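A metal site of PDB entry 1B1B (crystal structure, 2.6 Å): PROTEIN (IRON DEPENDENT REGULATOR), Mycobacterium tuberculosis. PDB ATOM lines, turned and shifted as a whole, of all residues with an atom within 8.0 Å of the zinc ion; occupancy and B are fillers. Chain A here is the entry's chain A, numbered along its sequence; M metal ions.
Residues that only touch the zinc ion: Glu 3 (3.6 Å).
Of the 22 residues printed, 5 come within 4 Å of the zinc ion.
The guanidinium group (NE) of Arg 13 lies within salt-bridge range of the side-chain carboxylate (OE1) of Glu 105 (3.6 Å).
A ring nitrogen (ND1) of His 79 lies within hydrogen-bond range of the side-chain carboxylate (OE1) of Glu 105 (2.5 Å).
A ring nitrogen (ND1) of His 106 sits at hydrogen-bond distance from the side-chain carboxylate (OE1) of Glu 9, at 2.8 Å.
The backbone carbonyl oxygen of Met 10 sits at hydrogen-bond distance from the side-chain hydroxyl of Thr 14, at 3.2 Å.
The guanidinium group (NE) of Arg 103 is in salt-bridge range of the side-chain carboxylate (OE2) of Glu 3, 3.1 Å away.
The zinc ion is bound by OE2 of Glu 105 (1.8 Å), O of Cys 102 (2.0 Å), NE2 of His 106 (2.4 Å) and SD of Met 10 (2.7 Å).
The zinc ion has four donor atoms within binding distance.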
ATOM      1  N   ASN A   2     -29.690 -15.936  -4.663  1.00  0.00           N
ATOM      2  CA  ASN A   2     -28.889 -15.418  -3.559  1.00  0.00           C
ATOM      3  C   ASN A   2     -28.403 -14.022  -3.832  1.00  0.00           C
ATOM      4  O   ASN A   2     -27.216 -13.734  -3.646  1.00  0.00           O
ATOM      5  CB  ASN A   2     -27.701 -16.347  -3.282  1.00  0.00           C
ATOM      6  CG  ASN A   2     -28.128 -17.776  -3.078  1.00  0.00           C
ATOM      7  OD1 ASN A   2     -27.701 -18.661  -3.818  1.00  0.00           O
ATOM      8  ND2 ASN A   2     -29.030 -17.981  -2.136  1.00  0.00           N
ATOM      9  N   GLU A   3     -29.295 -13.165  -4.317  1.00  0.00           N
ATOM     10  CA  GLU A   3     -28.954 -11.783  -4.614  1.00  0.00           C
ATOM     11  C   GLU A   3     -28.097 -11.673  -5.861  1.00  0.00           C
ATOM     12  O   GLU A   3     -27.918 -10.602  -6.421  1.00  0.00           O
ATOM     13  CB  GLU A   3     -28.319 -11.117  -3.401  1.00  0.00           C
ATOM     14  CG  GLU A   3     -29.272 -10.881  -2.196  1.00  0.00           C
ATOM     15  CD  GLU A   3     -30.025 -12.124  -1.749  1.00  0.00           C
ATOM     16  OE1 GLU A   3     -29.500 -12.880  -0.894  1.00  0.00           O
ATOM     17  OE2 GLU A   3     -31.150 -12.374  -2.260  1.00  0.00           O
ATOM     18  N   LEU A   4     -27.545 -12.813  -6.277  1.00  0.00           N
ATOM     19  CA  LEU A   4     -26.740 -12.924  -7.489  1.00  0.00           C
ATOM     20  C   LEU A   4     -27.726 -13.756  -8.311  1.00  0.00           C
ATOM     21  O   LEU A   4     -27.411 -14.833  -8.823  1.00  0.00           O
ATOM     22  CB  LEU A   4     -25.469 -13.719  -7.228  1.00  0.00           C
ATOM     23  N   VAL A   5     -28.955 -13.234  -8.409  1.00  0.00           N
ATOM     24  CA  VAL A   5     -30.056 -13.890  -9.087  1.00  0.00           C
ATOM     25  C   VAL A   5     -29.809 -14.350 -10.527  1.00  0.00           C
ATOM     26  O   VAL A   5     -30.585 -15.136 -11.071  1.00  0.00           O
ATOM     27  CB  VAL A   5     -31.411 -13.065  -8.936  1.00  0.00           C
ATOM     28  CG1 VAL A   5     -31.644 -12.710  -7.475  1.00  0.00           C
ATOM     29  CG2 VAL A   5     -31.357 -11.816  -9.709  1.00  0.00           C
ATOM     30  N   ASP A   6     -28.688 -13.920 -11.095  1.00  0.00           N
ATOM     31  CA  ASP A   6     -28.307 -14.289 -12.456  1.00  0.00           C
ATOM     32  C   ASP A   6     -26.778 -14.255 -12.538  1.00  0.00           C
ATOM     33  O   ASP A   6     -26.176 -13.174 -12.666  1.00  0.00           O
ATOM     34  CB  ASP A   6     -28.922 -13.313 -13.482  1.00  0.00           C
ATOM     35  CG  ASP A   6     -28.942 -13.853 -14.903  1.00  0.00           C
ATOM     36  OD1 ASP A   6     -28.118 -14.722 -15.277  1.00  0.00           O
ATOM     37  OD2 ASP A   6     -29.812 -13.401 -15.685  1.00  0.00           O
ATOM     38  N   THR A   7     -26.155 -15.421 -12.441  1.00  0.00           N
ATOM     39  CA  THR A   7     -24.697 -15.517 -12.491  1.00  0.00           C
ATOM     40  C   THR A   7     -24.128 -14.882 -13.756  1.00  0.00           C
ATOM     41  O   THR A   7     -23.308 -13.986 -13.659  1.00  0.00           O
ATOM     42  CB  THR A   7     -24.233 -16.967 -12.400  1.00  0.00           C
ATOM     43  OG1 THR A   7     -24.626 -17.664 -13.597  1.00  0.00           O
ATOM     44  CG2 THR A   7     -24.861 -17.642 -11.186  1.00  0.00           C
ATOM     45  N   GLU A   9     -25.097 -12.649 -15.687  1.00  0.00           N
ATOM     46  CA  GLU A   9     -25.133 -11.182 -15.604  1.00  0.00           C
ATOM     47  C   GLU A   9     -24.205 -10.665 -14.511  1.00  0.00           C
ATOM     48  O   GLU A   9     -23.576  -9.613 -14.676  1.00  0.00           O
ATOM     49  CB  GLU A   9     -26.552 -10.659 -15.433  1.00  0.00           C
ATOM     50  CG  GLU A   9     -27.449 -11.009 -16.645  1.00  0.00           C
ATOM     51  CD  GLU A   9     -28.862 -10.420 -16.550  1.00  0.00           C
ATOM     52  OE1 GLU A   9     -29.484 -10.491 -15.464  1.00  0.00           O
ATOM     53  OE2 GLU A   9     -29.360  -9.940 -17.570  1.00  0.00           O
ATOM     54  N   MET A  10     -24.064 -11.421 -13.416  1.00  0.00           N
ATOM     55  CA  MET A  10     -23.178 -10.984 -12.343  1.00  0.00           C
ATOM     56  C   MET A  10     -21.737 -10.934 -12.804  1.00  0.00           C
ATOM     57  O   MET A  10     -21.069  -9.924 -12.637  1.00  0.00           O
ATOM     58  CB  MET A  10     -23.309 -11.867 -11.120  1.00  0.00           C
ATOM     59  CG  MET A  10     -24.516 -11.526 -10.261  1.00  0.00           C
ATOM     60  SD  MET A  10     -24.847  -9.704 -10.066  1.00  0.00           S
ATOM     61  CE  MET A  10     -23.129  -9.073  -9.803  1.00  0.00           C
ATOM     62  N   ARG A  13     -21.225  -8.155 -15.100  1.00  0.00           N
ATOM     63  CA  ARG A  13     -21.344  -6.927 -14.330  1.00  0.00           C
ATOM     64  C   ARG A  13     -20.057  -6.639 -13.557  1.00  0.00           C
ATOM     65  O   ARG A  13     -19.427  -5.596 -13.745  1.00  0.00           O
ATOM     66  CB  ARG A  13     -22.540  -7.037 -13.379  1.00  0.00           C
ATOM     67  CG  ARG A  13     -23.311  -5.745 -13.194  1.00  0.00           C
ATOM     68  CD  ARG A  13     -22.645  -4.817 -12.179  1.00  0.00           C
ATOM     69  NE  ARG A  13     -23.441  -4.647 -10.969  1.00  0.00           N
ATOM     70  CZ  ARG A  13     -23.039  -4.940  -9.736  1.00  0.00           C
ATOM     71  NH1 ARG A  13     -21.838  -5.401  -9.507  1.00  0.00           N
ATOM     72  NH2 ARG A  13     -23.862  -4.741  -8.707  1.00  0.00           N
ATOM     73  N   THR A  14     -19.657  -7.598 -12.719  1.00  0.00           N
ATOM     74  CA  THR A  14     -18.447  -7.465 -11.918  1.00  0.00           C
ATOM     75  C   THR A  14     -17.225  -6.990 -12.716  1.00  0.00           C
ATOM     76  O   THR A  14     -16.368  -6.312 -12.172  1.00  0.00           O
ATOM     77  CB  THR A  14     -18.130  -8.791 -11.219  1.00  0.00           C
ATOM     78  OG1 THR A  14     -19.149  -9.052 -10.202  1.00  0.00           O
ATOM     79  CG2 THR A  14     -16.749  -8.764 -10.585  1.00  0.00           C
ATOM     80  N   LEU A  34     -17.744 -12.474  -5.872  1.00  0.00           N
ATOM     81  CA  LEU A  34     -19.009 -13.194  -5.984  1.00  0.00           C
ATOM     82  C   LEU A  34     -19.106 -14.419  -5.089  1.00  0.00           C
ATOM     83  O   LEU A  34     -20.123 -15.094  -5.069  1.00  0.00           O
ATOM     84  CB  LEU A  34     -19.231 -13.597  -7.439  1.00  0.00           C
ATOM     85  CG  LEU A  34     -19.114 -12.508  -8.506  1.00  0.00           C
ATOM     86  CD1 LEU A  34     -19.261 -13.105  -9.882  1.00  0.00           C
ATOM     87  CD2 LEU A  34     -20.169 -11.435  -8.291  1.00  0.00           C
ATOM     88  N   VAL A  75     -27.518  -4.192 -17.655  1.00  0.00           N
ATOM     89  CA  VAL A  75     -27.740  -4.629 -16.276  1.00  0.00           C
ATOM     90  C   VAL A  75     -27.287  -3.499 -15.323  1.00  0.00           C
ATOM     91  O   VAL A  75     -27.877  -3.305 -14.254  1.00  0.00           O
ATOM     92  CB  VAL A  75     -26.962  -5.937 -15.992  1.00  0.00           C
ATOM     93  CG1 VAL A  75     -27.084  -6.341 -14.528  1.00  0.00           C
ATOM     94  CG2 VAL A  75     -27.440  -7.036 -16.922  1.00  0.00           C
ATOM     95  N   HIS A  79     -29.635  -1.623 -12.915  1.00  0.00           N
ATOM     96  CA  HIS A  79     -29.125  -1.525 -11.563  1.00  0.00           C
ATOM     97  C   HIS A  79     -29.274  -0.096 -11.061  1.00  0.00           C
ATOM     98  O   HIS A  79     -29.971   0.183 -10.080  1.00  0.00           O
ATOM     99  CB  HIS A  79     -27.644  -1.908 -11.592  1.00  0.00           C
ATOM    100  CG  HIS A  79     -26.969  -1.858 -10.268  1.00  0.00           C
ATOM    101  ND1 HIS A  79     -26.583  -2.997  -9.621  1.00  0.00           N
ATOM    102  CD2 HIS A  79     -26.762  -0.793  -9.456  1.00  0.00           C
ATOM    103  CE1 HIS A  79     -26.143  -2.605  -8.440  1.00  0.00           C
ATOM    104  NE2 HIS A  79     -26.218  -1.283  -8.271  1.00  0.00           N
ATOM    105  N   HIS A  98     -28.254  -0.259  -2.520  1.00  0.00           N
ATOM    106  CA  HIS A  98     -27.358  -1.094  -3.334  1.00  0.00           C
ATOM    107  C   HIS A  98     -27.680  -2.580  -3.408  1.00  0.00           C
ATOM    108  O   HIS A  98     -27.742  -3.128  -4.510  1.00  0.00           O
ATOM    109  CB  HIS A  98     -25.913  -0.947  -2.859  1.00  0.00           C
ATOM    110  CG  HIS A  98     -24.951  -1.812  -3.640  1.00  0.00           C
ATOM    111  ND1 HIS A  98     -24.626  -1.513  -4.954  1.00  0.00           N
ATOM    112  CD2 HIS A  98     -24.293  -2.917  -3.274  1.00  0.00           C
ATOM    113  CE1 HIS A  98     -23.764  -2.433  -5.310  1.00  0.00           C
ATOM    114  NE2 HIS A  98     -23.525  -3.309  -4.343  1.00  0.00           N
ATOM    115  N   ALA A  99     -27.757  -3.217  -2.237  1.00  0.00           N
ATOM    116  CA  ALA A  99     -28.048  -4.640  -2.172  1.00  0.00           C
ATOM    117  C   ALA A  99     -29.419  -4.950  -2.766  1.00  0.00           C
ATOM    118  O   ALA A  99     -29.637  -6.030  -3.277  1.00  0.00           O
ATOM    119  CB  ALA A  99     -27.977  -5.134  -0.760  1.00  0.00           C
ATOM    120  N   GLU A 100     -30.301  -3.963  -2.699  1.00  0.00           N
ATOM    121  CA  GLU A 100     -31.657  -4.075  -3.250  1.00  0.00           C
ATOM    122  C   GLU A 100     -31.605  -4.052  -4.774  1.00  0.00           C
ATOM    123  O   GLU A 100     -32.102  -4.969  -5.444  1.00  0.00           O
ATOM    124  CB  GLU A 100     -32.552  -2.947  -2.727  1.00  0.00           C
ATOM    125  CG  GLU A 100     -34.033  -3.063  -3.122  1.00  0.00           C
ATOM    126  CD  GLU A 100     -34.810  -4.025  -2.246  1.00  0.00           C
ATOM    127  OE1 GLU A 100     -34.549  -4.079  -1.044  1.00  0.00           O
ATOM    128  OE2 GLU A 100     -35.687  -4.748  -2.758  1.00  0.00           O
ATOM    129  N   ALA A 101     -30.988  -2.995  -5.332  1.00  0.00           N
ATOM    130  CA  ALA A 101     -30.833  -2.808  -6.770  1.00  0.00           C
ATOM    131  C   ALA A 101     -29.985  -3.924  -7.385  1.00  0.00           C
ATOM    132  O   ALA A 101     -30.161  -4.262  -8.555  1.00  0.00           O
ATOM    133  CB  ALA A 101     -30.203  -1.483  -7.041  1.00  0.00           C
ATOM    134  N   CYS A 102     -29.095  -4.502  -6.570  1.00  0.00           N
ATOM    135  CA  CYS A 102     -28.203  -5.602  -6.951  1.00  0.00           C
ATOM    136  C   CYS A 102     -29.050  -6.817  -7.426  1.00  0.00           C
ATOM    137  O   CYS A 102     -28.588  -7.650  -8.209  1.00  0.00           O
ATOM    138  CB  CYS A 102     -27.319  -5.964  -5.746  1.00  0.00           C
ATOM    139  SG  CYS A 102     -25.861  -7.036  -6.032  1.00  0.00           S
ATOM    140  N   ARG A 103     -30.287  -6.904  -6.947  1.00  0.00           N
ATOM    141  CA  ARG A 103     -31.189  -7.979  -7.312  1.00  0.00           C
ATOM    142  C   ARG A 103     -32.159  -7.556  -8.411  1.00  0.00           C
ATOM    143  O   ARG A 103     -32.239  -8.183  -9.464  1.00  0.00           O
ATOM    144  CB  ARG A 103     -31.948  -8.427  -6.086  1.00  0.00           C
ATOM    145  CG  ARG A 103     -31.096  -9.239  -5.171  1.00  0.00           C
ATOM    146  CD  ARG A 103     -31.904 -10.080  -4.221  1.00  0.00           C
ATOM    147  NE  ARG A 103     -31.939  -9.451  -2.925  1.00  0.00           N
ATOM    148  CZ  ARG A 103     -32.888  -8.612  -2.559  1.00  0.00           C
ATOM    149  NH1 ARG A 103     -33.860  -8.336  -3.416  1.00  0.00           N
ATOM    150  NH2 ARG A 103     -32.882  -8.031  -1.366  1.00  0.00           N
ATOM    151  N   TRP A 104     -32.892  -6.486  -8.142  1.00  0.00           N
ATOM    152  CA  TRP A 104     -33.884  -5.959  -9.075  1.00  0.00           C
ATOM    153  C   TRP A 104     -33.304  -5.774 -10.466  1.00  0.00           C
ATOM    154  O   TRP A 104     -34.006  -5.916 -11.455  1.00  0.00           O
ATOM    155  CB  TRP A 104     -34.472  -4.637  -8.568  1.00  0.00           C
ATOM    156  CG  TRP A 104     -35.334  -4.792  -7.322  1.00  0.00           C
ATOM    157  CD1 TRP A 104     -35.367  -5.846  -6.461  1.00  0.00           C
ATOM    158  CD2 TRP A 104     -36.268  -3.831  -6.818  1.00  0.00           C
ATOM    159  NE1 TRP A 104     -36.259  -5.597  -5.456  1.00  0.00           N
ATOM    160  CE2 TRP A 104     -36.833  -4.367  -5.644  1.00  0.00           C
ATOM    161  CE3 TRP A 104     -36.687  -2.556  -7.236  1.00  0.00           C
ATOM    162  CZ2 TRP A 104     -37.775  -3.689  -4.870  1.00  0.00           C
ATOM    163  CZ3 TRP A 104     -37.619  -1.872  -6.482  1.00  0.00           C
ATOM    164  CH2 TRP A 104     -38.166  -2.454  -5.312  1.00  0.00           C
ATOM    165  N   GLU A 105     -31.995  -5.507 -10.526  1.00  0.00           N
ATOM    166  CA  GLU A 105     -31.311  -5.313 -11.806  1.00  0.00           C
ATOM    167  C   GLU A 105     -31.493  -6.482 -12.762  1.00  0.00           C
ATOM    168  O   GLU A 105     -31.515  -6.293 -13.987  1.00  0.00           O
ATOM    169  CB  GLU A 105     -29.801  -5.057 -11.585  1.00  0.00           C
ATOM    170  CG  GLU A 105     -29.124  -6.098 -10.735  1.00  0.00           C
ATOM    171  CD  GLU A 105     -27.575  -5.967 -10.725  1.00  0.00           C
ATOM    172  OE1 GLU A 105     -27.035  -4.947 -11.140  1.00  0.00           O
ATOM    173  OE2 GLU A 105     -26.953  -7.014 -10.224  1.00  0.00           O
ATOM    174  N   HIS A 106     -31.623  -7.705 -12.220  1.00  0.00           N
ATOM    175  CA  HIS A 106     -31.779  -8.887 -13.058  1.00  0.00           C
ATOM    176  C   HIS A 106     -33.212  -9.124 -13.453  1.00  0.00           C
ATOM    177  O   HIS A 106     -33.497 -10.002 -14.281  1.00  0.00           O
ATOM    178  CB  HIS A 106     -31.254 -10.148 -12.361  1.00  0.00           C
ATOM    179  CG  HIS A 106     -29.831 -10.043 -11.889  1.00  0.00           C
ATOM    180  ND1 HIS A 106     -28.779 -10.286 -12.747  1.00  0.00           N
ATOM    181  CD2 HIS A 106     -29.347  -9.723 -10.677  1.00  0.00           C
ATOM    182  CE1 HIS A 106     -27.699 -10.101 -12.014  1.00  0.00           C
ATOM    183  NE2 HIS A 106     -27.960  -9.758 -10.763  1.00  0.00           N
HETATM  184 ZN    ZN M   1     -26.955  -8.415  -9.048  1.00  0.00          ZN
